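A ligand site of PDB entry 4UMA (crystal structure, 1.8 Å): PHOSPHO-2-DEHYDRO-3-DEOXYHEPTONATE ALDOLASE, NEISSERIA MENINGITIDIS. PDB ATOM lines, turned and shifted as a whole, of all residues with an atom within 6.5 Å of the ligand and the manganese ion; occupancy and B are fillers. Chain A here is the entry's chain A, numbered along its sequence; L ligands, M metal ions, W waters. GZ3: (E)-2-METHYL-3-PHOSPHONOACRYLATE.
Tyr 96 touches the ligand. Pro 100 touches the ligand. Gly 165 touches the ligand. Hydrophobic or aromatic side chains within 4 Å of the ligand: Tyr 96, Pro 100, Ala 166 and His 270. Within 4 Å of the ligand: Cys 63, Arg 94, Tyr 96, Lys 99, Pro 100, Gly 165, Ala 166, Arg 167, Lys 188, Arg 236, His 270, Glu 304 and Asp 324. Along chain A the residues within 4 Å of the ligand span positions 63 to 324. The nearest printed residue that does not touch the ligand is Glu 145 (4.4 Å).
The side-chain amino group (NZ) of Lys 99 lies within salt-bridge range of an oxygen (OAB) of the ligand (3.8 Å). The side-chain amino group (NZ) of Lys 188 lies within salt-bridge range of an oxygen (OAE) of the ligand (2.7 Å). NE of Arg 236 is in salt-bridge range of OAE of the ligand (2.8 Å). The guanidinium group (NH1) of Arg 167 is in salt-bridge range of an oxygen (OAF) of the ligand (2.8 Å). An oxygen (OAC) of the ligand is in hydrogen-bond range of the backbone NH of Ala 166 (2.9 Å). An oxygen (OAB) of the ligand is in salt-bridge range of the guanidinium group (NH2) of Arg 94 (2.9 Å).
OE1 of Glu 304 sits at hydrogen-bond distance from OG of Ser 269 (2.7 Å). The side-chain carboxylate (OD2) of Asp 267 lies within hydrogen-bond range of a ring nitrogen (ND1) of His 270 (2.7 Å). The guanidinium group (NH2) of Arg 94 lies within hydrogen-bond range of the backbone carbonyl oxygen (O) of Cys 63 (3.0 Å). The side-chain sulfur (SG) of Cys 63 lies close to the side-chain hydroxyl (OG1) of Thr 323 (3.0 Å). NZ of Lys 188 is in salt-bridge range of OD2 of Asp 267, at 2.9 Å. O of Ile 164 lies close to N of Lys 188. The backbone NH (N) of Arg 236 is in hydrogen-bond range of the side-chain amide oxygen (OD1) of Asn 189, 2.8 Å away. O of Pro 62 lies within hydrogen-bond range of NE of Arg 94.
The manganese ion is bound by the side-chain carboxylate (OE2) of Glu 304, the side-chain carboxylate (OD2) of Asp 324, an oxygen (OAD) of the ligand, a ring nitrogen (NE2) of His 270 and the side-chain sulfur (SG) of Cys 63. The manganese ion has five donor atoms within binding distance.
Water W2 lies within hydrogen-bond range of OAC of the ligand, NH1 of Arg 167 and N of Ala 166. Water W4 lies within hydrogen-bond range of OAF of the ligand (2.7 Å) and NH2 of Arg 167 (2.9 Å). Water W6 bridges the side-chain carboxylate (OE1) of Glu 145 (2.8 Å) and an oxygen (OAC) of the ligand (2.9 Å). Water W3 lies within hydrogen-bond range of OH of Tyr 96, OAB of the ligand and NZ of Lys 188.
The nearest printed residue that does not touch the manganese ion is Arg 94 (4.2 Å).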
ATOM      1  N   PRO A  62      -7.371   3.293  -2.604  1.00  0.00           N
ATOM      2  CA  PRO A  62      -7.228   4.139  -3.779  1.00  0.00           C
ATOM      3  C   PRO A  62      -5.787   4.236  -4.295  1.00  0.00           C
ATOM      4  O   PRO A  62      -4.811   4.040  -3.568  1.00  0.00           O
ATOM      5  CB  PRO A  62      -7.705   5.500  -3.281  1.00  0.00           C
ATOM      6  CG  PRO A  62      -8.695   5.170  -2.202  1.00  0.00           C
ATOM      7  CD  PRO A  62      -8.160   3.929  -1.541  1.00  0.00           C
ATOM      8  N   CYS A  63      -5.677   4.528  -5.580  1.00  0.00           N
ATOM      9  CA  CYS A  63      -4.393   4.820  -6.183  1.00  0.00           C
ATOM     10  C   CYS A  63      -3.809   6.038  -5.417  1.00  0.00           C
ATOM     11  O   CYS A  63      -2.643   6.036  -4.983  1.00  0.00           O
ATOM     12  CB  CYS A  63      -4.547   5.101  -7.664  1.00  0.00           C
ATOM     13  SG  CYS A  63      -2.966   5.627  -8.401  1.00  0.00           S
ATOM     14  N   SER A  64      -4.648   7.046  -5.244  1.00  0.00           N
ATOM     15  CA  SER A  64      -4.299   8.288  -4.565  1.00  0.00           C
ATOM     16  C   SER A  64      -5.472   8.774  -3.735  1.00  0.00           C
ATOM     17  O   SER A  64      -6.622   8.562  -4.104  1.00  0.00           O
ATOM     18  CB  SER A  64      -3.940   9.368  -5.611  1.00  0.00           C
ATOM     19  OG  SER A  64      -5.043   9.653  -6.482  1.00  0.00           O
ATOM     20  N   ARG A  94      -4.437   1.592   1.567  1.00  0.00           N
ATOM     21  CA  ARG A  94      -3.632   2.494   0.746  1.00  0.00           C
ATOM     22  C   ARG A  94      -4.088   3.901   1.033  1.00  0.00           C
ATOM     23  O   ARG A  94      -5.242   4.254   0.754  1.00  0.00           O
ATOM     24  CB  ARG A  94      -3.797   2.256  -0.765  1.00  0.00           C
ATOM     25  CG  ARG A  94      -3.136   0.970  -1.301  1.00  0.00           C
ATOM     26  CD  ARG A  94      -3.325   0.781  -2.813  1.00  0.00           C
ATOM     27  NE  ARG A  94      -2.906   1.973  -3.566  1.00  0.00           N
ATOM     28  CZ  ARG A  94      -1.804   2.092  -4.316  1.00  0.00           C
ATOM     29  NH1 ARG A  94      -1.011   1.049  -4.582  1.00  0.00           N
ATOM     30  NH2 ARG A  94      -1.517   3.256  -4.844  1.00  0.00           N
ATOM     31  N   TYR A  96      -2.207   6.987  -0.124  1.00  0.00           N
ATOM     32  CA  TYR A  96      -1.064   7.519  -0.900  1.00  0.00           C
ATOM     33  C   TYR A  96      -1.240   9.005  -1.117  1.00  0.00           C
ATOM     34  O   TYR A  96      -2.243   9.464  -1.725  1.00  0.00           O
ATOM     35  CB  TYR A  96      -0.943   6.822  -2.232  1.00  0.00           C
ATOM     36  CG  TYR A  96      -0.227   5.481  -2.256  1.00  0.00           C
ATOM     37  CD1 TYR A  96      -0.536   4.471  -1.356  1.00  0.00           C
ATOM     38  CD2 TYR A  96       0.803   5.231  -3.197  1.00  0.00           C
ATOM     39  CE1 TYR A  96       0.113   3.240  -1.385  1.00  0.00           C
ATOM     40  CE2 TYR A  96       1.424   4.001  -3.249  1.00  0.00           C
ATOM     41  CZ  TYR A  96       1.074   3.002  -2.378  1.00  0.00           C
ATOM     42  OH  TYR A  96       1.704   1.780  -2.400  1.00  0.00           O
ATOM     43  N   LYS A  99       2.456  11.115  -5.566  1.00  0.00           N
ATOM     44  CA  LYS A  99       2.352  10.398  -6.813  1.00  0.00           C
ATOM     45  C   LYS A  99       3.493  10.774  -7.797  1.00  0.00           C
ATOM     46  O   LYS A  99       3.642  11.944  -8.150  1.00  0.00           O
ATOM     47  CB  LYS A  99       1.041  10.687  -7.499  1.00  0.00           C
ATOM     48  CG  LYS A  99      -0.213  10.418  -6.642  1.00  0.00           C
ATOM     49  CD  LYS A  99      -0.254   9.030  -6.012  1.00  0.00           C
ATOM     50  CE  LYS A  99      -0.384   7.897  -7.039  1.00  0.00           C
ATOM     51  NZ  LYS A  99      -0.228   6.534  -6.443  1.00  0.00           N
ATOM     52  N   PRO A 100       4.214   9.775  -8.269  1.00  0.00           N
ATOM     53  CA  PRO A 100       5.232  10.003  -9.301  1.00  0.00           C
ATOM     54  C   PRO A 100       4.580  10.070 -10.693  1.00  0.00           C
ATOM     55  O   PRO A 100       3.840   9.152 -11.060  1.00  0.00           O
ATOM     56  CB  PRO A 100       6.125   8.784  -9.169  1.00  0.00           C
ATOM     57  CG  PRO A 100       5.188   7.664  -8.689  1.00  0.00           C
ATOM     58  CD  PRO A 100       4.142   8.352  -7.862  1.00  0.00           C
ATOM     59  N   GLU A 145       3.194   5.507  -0.314  1.00  0.00           N
ATOM     60  CA  GLU A 145       4.475   5.533  -0.996  1.00  0.00           C
ATOM     61  C   GLU A 145       5.229   6.729  -0.438  1.00  0.00           C
ATOM     62  O   GLU A 145       4.725   7.866  -0.458  1.00  0.00           O
ATOM     63  CB  GLU A 145       4.372   5.659  -2.534  1.00  0.00           C
ATOM     64  CG  GLU A 145       5.755   5.944  -3.156  1.00  0.00           C
ATOM     65  CD  GLU A 145       5.816   6.080  -4.667  1.00  0.00           C
ATOM     66  OE1 GLU A 145       4.838   5.725  -5.397  1.00  0.00           O
ATOM     67  OE2 GLU A 145       6.909   6.519  -5.121  1.00  0.00           O
ATOM     68  N   ILE A 164       8.454   2.025  -1.596  1.00  0.00           N
ATOM     69  CA  ILE A 164       9.333   2.858  -2.422  1.00  0.00           C
ATOM     70  C   ILE A 164       8.991   2.431  -3.843  1.00  0.00           C
ATOM     71  O   ILE A 164       9.058   1.243  -4.190  1.00  0.00           O
ATOM     72  CB  ILE A 164      10.857   2.648  -2.105  1.00  0.00           C
ATOM     73  CG1 ILE A 164      11.185   3.012  -0.633  1.00  0.00           C
ATOM     74  CG2 ILE A 164      11.695   3.460  -3.077  1.00  0.00           C
ATOM     75  CD1 ILE A 164      10.907   4.443  -0.229  1.00  0.00           C
ATOM     76  N   GLY A 165       8.618   3.394  -4.663  1.00  0.00           N
ATOM     77  CA  GLY A 165       8.100   3.098  -5.992  1.00  0.00           C
ATOM     78  C   GLY A 165       9.038   2.479  -6.972  1.00  0.00           C
ATOM     79  O   GLY A 165      10.275   2.557  -6.825  1.00  0.00           O
ATOM     80  N   ALA A 166       8.471   1.943  -8.032  1.00  0.00           N
ATOM     81  CA  ALA A 166       9.241   1.388  -9.115  1.00  0.00           C
ATOM     82  C   ALA A 166      10.245   2.374  -9.665  1.00  0.00           C
ATOM     83  O   ALA A 166      11.360   2.005 -10.033  1.00  0.00           O
ATOM     84  CB  ALA A 166       8.317   0.929 -10.213  1.00  0.00           C
ATOM     85  N   ARG A 167       9.852   3.645  -9.719  1.00  0.00           N
ATOM     86  CA  ARG A 167      10.691   4.702 -10.331  1.00  0.00           C
ATOM     87  C   ARG A 167      11.793   5.238  -9.437  1.00  0.00           C
ATOM     88  O   ARG A 167      12.645   6.024  -9.893  1.00  0.00           O
ATOM     89  CB  ARG A 167       9.798   5.845 -10.801  1.00  0.00           C
ATOM     90  CG  ARG A 167       8.852   5.396 -11.902  1.00  0.00           C
ATOM     91  CD  ARG A 167       7.769   6.434 -12.209  1.00  0.00           C
ATOM     92  NE  ARG A 167       6.792   5.882 -13.141  1.00  0.00           N
ATOM     93  CZ  ARG A 167       5.799   5.081 -12.780  1.00  0.00           C
ATOM     94  NH1 ARG A 167       5.666   4.710 -11.514  1.00  0.00           N
ATOM     95  NH2 ARG A 167       4.972   4.590 -13.689  1.00  0.00           N
ATOM     96  N   THR A 168      11.733   4.858  -8.171  1.00  0.00           N
ATOM     97  CA  THR A 168      12.654   5.333  -7.155  1.00  0.00           C
ATOM     98  C   THR A 168      13.388   4.246  -6.364  1.00  0.00           C
ATOM     99  O   THR A 168      14.197   4.539  -5.505  1.00  0.00           O
ATOM    100  CB  THR A 168      11.922   6.267  -6.183  1.00  0.00           C
ATOM    101  OG1 THR A 168      10.626   5.737  -5.905  1.00  0.00           O
ATOM    102  CG2 THR A 168      11.770   7.641  -6.800  1.00  0.00           C
ATOM    103  N   LYS A 188       9.811  -1.916  -5.032  1.00  0.00           N
ATOM    104  CA  LYS A 188       9.196  -2.433  -6.223  1.00  0.00           C
ATOM    105  C   LYS A 188      10.225  -2.713  -7.311  1.00  0.00           C
ATOM    106  O   LYS A 188      11.203  -1.988  -7.443  1.00  0.00           O
ATOM    107  CB  LYS A 188       8.159  -1.423  -6.701  1.00  0.00           C
ATOM    108  CG  LYS A 188       7.163  -1.084  -5.598  1.00  0.00           C
ATOM    109  CD  LYS A 188       5.923  -0.403  -6.133  1.00  0.00           C
ATOM    110  CE  LYS A 188       4.779  -1.404  -6.253  1.00  0.00           C
ATOM    111  NZ  LYS A 188       3.609  -0.737  -6.872  1.00  0.00           N
ATOM    112  N   ASN A 189       9.964  -3.723  -8.125  1.00  0.00           N
ATOM    113  CA  ASN A 189      10.772  -3.908  -9.321  1.00  0.00           C
ATOM    114  C   ASN A 189      10.653  -2.693 -10.240  1.00  0.00           C
ATOM    115  O   ASN A 189       9.709  -1.913 -10.134  1.00  0.00           O
ATOM    116  CB  ASN A 189      10.482  -5.227 -10.022  1.00  0.00           C
ATOM    117  CG  ASN A 189       9.081  -5.284 -10.663  1.00  0.00           C
ATOM    118  OD1 ASN A 189       8.225  -6.022 -10.182  1.00  0.00           O
ATOM    119  ND2 ASN A 189       8.884  -4.588 -11.771  1.00  0.00           N
ATOM    120  N   THR A 191      10.379  -0.232 -13.682  1.00  0.00           N
ATOM    121  CA  THR A 191       9.237  -0.097 -14.563  1.00  0.00           C
ATOM    122  C   THR A 191       9.276  -0.973 -15.800  1.00  0.00           C
ATOM    123  O   THR A 191       8.243  -1.259 -16.385  1.00  0.00           O
ATOM    124  CB  THR A 191       8.973   1.371 -14.975  1.00  0.00           C
ATOM    125  OG1 THR A 191      10.175   1.927 -15.506  1.00  0.00           O
ATOM    126  CG2 THR A 191       8.533   2.145 -13.805  1.00  0.00           C
ATOM    127  N   ARG A 236       5.518  -5.960  -9.487  1.00  0.00           N
ATOM    128  CA  ARG A 236       4.466  -5.056 -10.031  1.00  0.00           C
ATOM    129  C   ARG A 236       4.423  -4.981 -11.547  1.00  0.00           C
ATOM    130  O   ARG A 236       3.822  -4.068 -12.116  1.00  0.00           O
ATOM    131  CB  ARG A 236       4.553  -3.654  -9.412  1.00  0.00           C
ATOM    132  CG  ARG A 236       5.915  -2.947  -9.478  1.00  0.00           C
ATOM    133  CD  ARG A 236       6.242  -2.453 -10.887  1.00  0.00           C
ATOM    134  NE  ARG A 236       5.548  -1.207 -11.230  1.00  0.00           N
ATOM    135  CZ  ARG A 236       5.482  -0.692 -12.450  1.00  0.00           C
ATOM    136  NH1 ARG A 236       5.988  -1.324 -13.483  1.00  0.00           N
ATOM    137  NH2 ARG A 236       4.887   0.476 -12.639  1.00  0.00           N
ATOM    138  N   ASP A 267       1.841  -7.015  -6.509  1.00  0.00           N
ATOM    139  CA  ASP A 267       0.887  -5.951  -6.872  1.00  0.00           C
ATOM    140  C   ASP A 267      -0.036  -6.469  -7.974  1.00  0.00           C
ATOM    141  O   ASP A 267       0.424  -6.880  -9.031  1.00  0.00           O
ATOM    142  CB  ASP A 267       1.686  -4.733  -7.348  1.00  0.00           C
ATOM    143  CG  ASP A 267       0.826  -3.476  -7.580  1.00  0.00           C
ATOM    144  OD1 ASP A 267      -0.435  -3.492  -7.476  1.00  0.00           O
ATOM    145  OD2 ASP A 267       1.451  -2.446  -7.850  1.00  0.00           O
ATOM    146  N   SER A 269      -2.201  -4.543  -9.474  1.00  0.00           N
ATOM    147  CA  SER A 269      -2.412  -3.411 -10.362  1.00  0.00           C
ATOM    148  C   SER A 269      -1.221  -3.051 -11.246  1.00  0.00           C
ATOM    149  O   SER A 269      -0.293  -3.838 -11.410  1.00  0.00           O
ATOM    150  CB  SER A 269      -2.889  -2.189  -9.591  1.00  0.00           C
ATOM    151  OG  SER A 269      -3.570  -1.298 -10.441  1.00  0.00           O
ATOM    152  N   HIS A 270      -1.290  -1.877 -11.849  1.00  0.00           N
ATOM    153  CA  HIS A 270      -0.170  -1.317 -12.595  1.00  0.00           C
ATOM    154  C   HIS A 270       0.286  -2.234 -13.726  1.00  0.00           C
ATOM    155  O   HIS A 270      -0.527  -2.651 -14.540  1.00  0.00           O
ATOM    156  CB  HIS A 270       0.947  -0.927 -11.631  1.00  0.00           C
ATOM    157  CG  HIS A 270       0.486   0.004 -10.550  1.00  0.00           C
ATOM    158  ND1 HIS A 270       0.335  -0.391  -9.239  1.00  0.00           N
ATOM    159  CD2 HIS A 270       0.071   1.295 -10.606  1.00  0.00           C
ATOM    160  CE1 HIS A 270      -0.121   0.626  -8.529  1.00  0.00           C
ATOM    161  NE2 HIS A 270      -0.284   1.652  -9.333  1.00  0.00           N
ATOM    162  N   ALA A 271       1.580  -2.522 -13.786  1.00  0.00           N
ATOM    163  CA  ALA A 271       2.122  -3.341 -14.863  1.00  0.00           C
ATOM    164  C   ALA A 271       1.574  -4.771 -14.881  1.00  0.00           C
ATOM    165  O   ALA A 271       1.624  -5.441 -15.909  1.00  0.00           O
ATOM    166  CB  ALA A 271       3.643  -3.351 -14.824  1.00  0.00           C
ATOM    167  N   MET A 302      -1.103  -6.240  -3.290  1.00  0.00           N
ATOM    168  CA  MET A 302      -1.574  -4.867  -3.387  1.00  0.00           C
ATOM    169  C   MET A 302      -2.686  -4.804  -4.385  1.00  0.00           C
ATOM    170  O   MET A 302      -2.649  -5.475  -5.389  1.00  0.00           O
ATOM    171  CB  MET A 302      -0.501  -3.877  -3.842  1.00  0.00           C
ATOM    172  CG  MET A 302       0.806  -4.018  -3.113  1.00  0.00           C
ATOM    173  SD  MET A 302       2.028  -2.833  -3.755  1.00  0.00           S
ATOM    174  CE  MET A 302       1.379  -1.286  -3.216  1.00  0.00           C
ATOM    175  N   GLU A 304      -5.645  -1.872  -6.101  1.00  0.00           N
ATOM    176  CA  GLU A 304      -6.133  -0.515  -6.257  1.00  0.00           C
ATOM    177  C   GLU A 304      -7.654  -0.571  -6.342  1.00  0.00           C
ATOM    178  O   GLU A 304      -8.232  -1.115  -7.295  1.00  0.00           O
ATOM    179  CB  GLU A 304      -5.503   0.190  -7.458  1.00  0.00           C
ATOM    180  CG  GLU A 304      -4.087   0.621  -7.151  1.00  0.00           C
ATOM    181  CD  GLU A 304      -3.399   1.466  -8.203  1.00  0.00           C
ATOM    182  OE1 GLU A 304      -3.477   1.149  -9.421  1.00  0.00           O
ATOM    183  OE2 GLU A 304      -2.823   2.520  -7.811  1.00  0.00           O
ATOM    184  N   THR A 323      -6.518   9.316 -10.458  1.00  0.00           N
ATOM    185  CA  THR A 323      -5.253   8.810 -10.973  1.00  0.00           C
ATOM    186  C   THR A 323      -5.473   7.438 -11.614  1.00  0.00           C
ATOM    187  O   THR A 323      -6.299   7.337 -12.508  1.00  0.00           O
ATOM    188  CB  THR A 323      -4.126   8.813  -9.912  1.00  0.00           C
ATOM    189  OG1 THR A 323      -4.565   8.143  -8.733  1.00  0.00           O
ATOM    190  CG2 THR A 323      -3.752  10.238  -9.562  1.00  0.00           C
ATOM    191  N   ASP A 324      -4.772   6.376 -11.188  1.00  0.00           N
ATOM    192  CA  ASP A 324      -4.975   5.107 -11.869  1.00  0.00           C
ATOM    193  C   ASP A 324      -6.395   4.585 -11.585  1.00  0.00           C
ATOM    194  O   ASP A 324      -6.928   4.810 -10.478  1.00  0.00           O
ATOM    195  CB  ASP A 324      -3.939   4.059 -11.434  1.00  0.00           C
ATOM    196  CG  ASP A 324      -2.506   4.499 -11.685  1.00  0.00           C
ATOM    197  OD1 ASP A 324      -2.272   5.233 -12.664  1.00  0.00           O
ATOM    198  OD2 ASP A 324      -1.629   4.106 -10.890  1.00  0.00           O
ATOM    199  N   ALA A 325      -6.980   3.881 -12.547  1.00  0.00           N
ATOM    200  CA  ALA A 325      -8.287   3.309 -12.383  1.00  0.00           C
ATOM    201  C   ALA A 325      -8.271   2.221 -11.301  1.00  0.00           C
ATOM    202  O   ALA A 325      -7.308   1.456 -11.192  1.00  0.00           O
ATOM    203  CB  ALA A 325      -8.822   2.760 -13.693  1.00  0.00           C
HETATM  204  CAI GZ3 L   1       0.997   3.666  -7.601  1.00  0.00           C
HETATM  205  OAB GZ3 L   1       0.716   2.876  -6.684  1.00  0.00           O
HETATM  206  OAD GZ3 L   1       0.215   4.539  -7.933  1.00  0.00           O
HETATM  207  CAH GZ3 L   1       2.312   3.578  -8.363  1.00  0.00           C
HETATM  208  CAA GZ3 L   1       2.715   4.731  -9.281  1.00  0.00           C
HETATM  209  CAG GZ3 L   1       2.969   2.273  -8.336  1.00  0.00           C
HETATM  210  PAJ GZ3 L   1       4.553   1.931  -9.130  1.00  0.00           P
HETATM  211  OAE GZ3 L   1       4.668   0.359  -9.141  1.00  0.00           O
HETATM  212  OAF GZ3 L   1       4.424   2.323 -10.621  1.00  0.00           O
HETATM  213  OAC GZ3 L   1       5.720   2.591  -8.434  1.00  0.00           O
HETATM  214 MN    MN M   1      -1.593   3.543  -8.987  1.00  0.00          MN
HETATM  215  O   HOH W   1       0.861   5.336 -11.604  1.00  0.00           O
HETATM  216  O   HOH W   2       7.157   4.713  -9.077  1.00  0.00           O
HETATM  217  O   HOH W   3       2.703   1.436  -5.017  1.00  0.00           O
HETATM  218  O   HOH W   4       2.688   3.274 -12.414  1.00  0.00           O
HETATM  219  O   HOH W   5       1.524   7.888 -10.107  1.00  0.00           O
HETATM  220  O   HOH W   6       4.839   2.969  -5.692  1.00  0.00           O
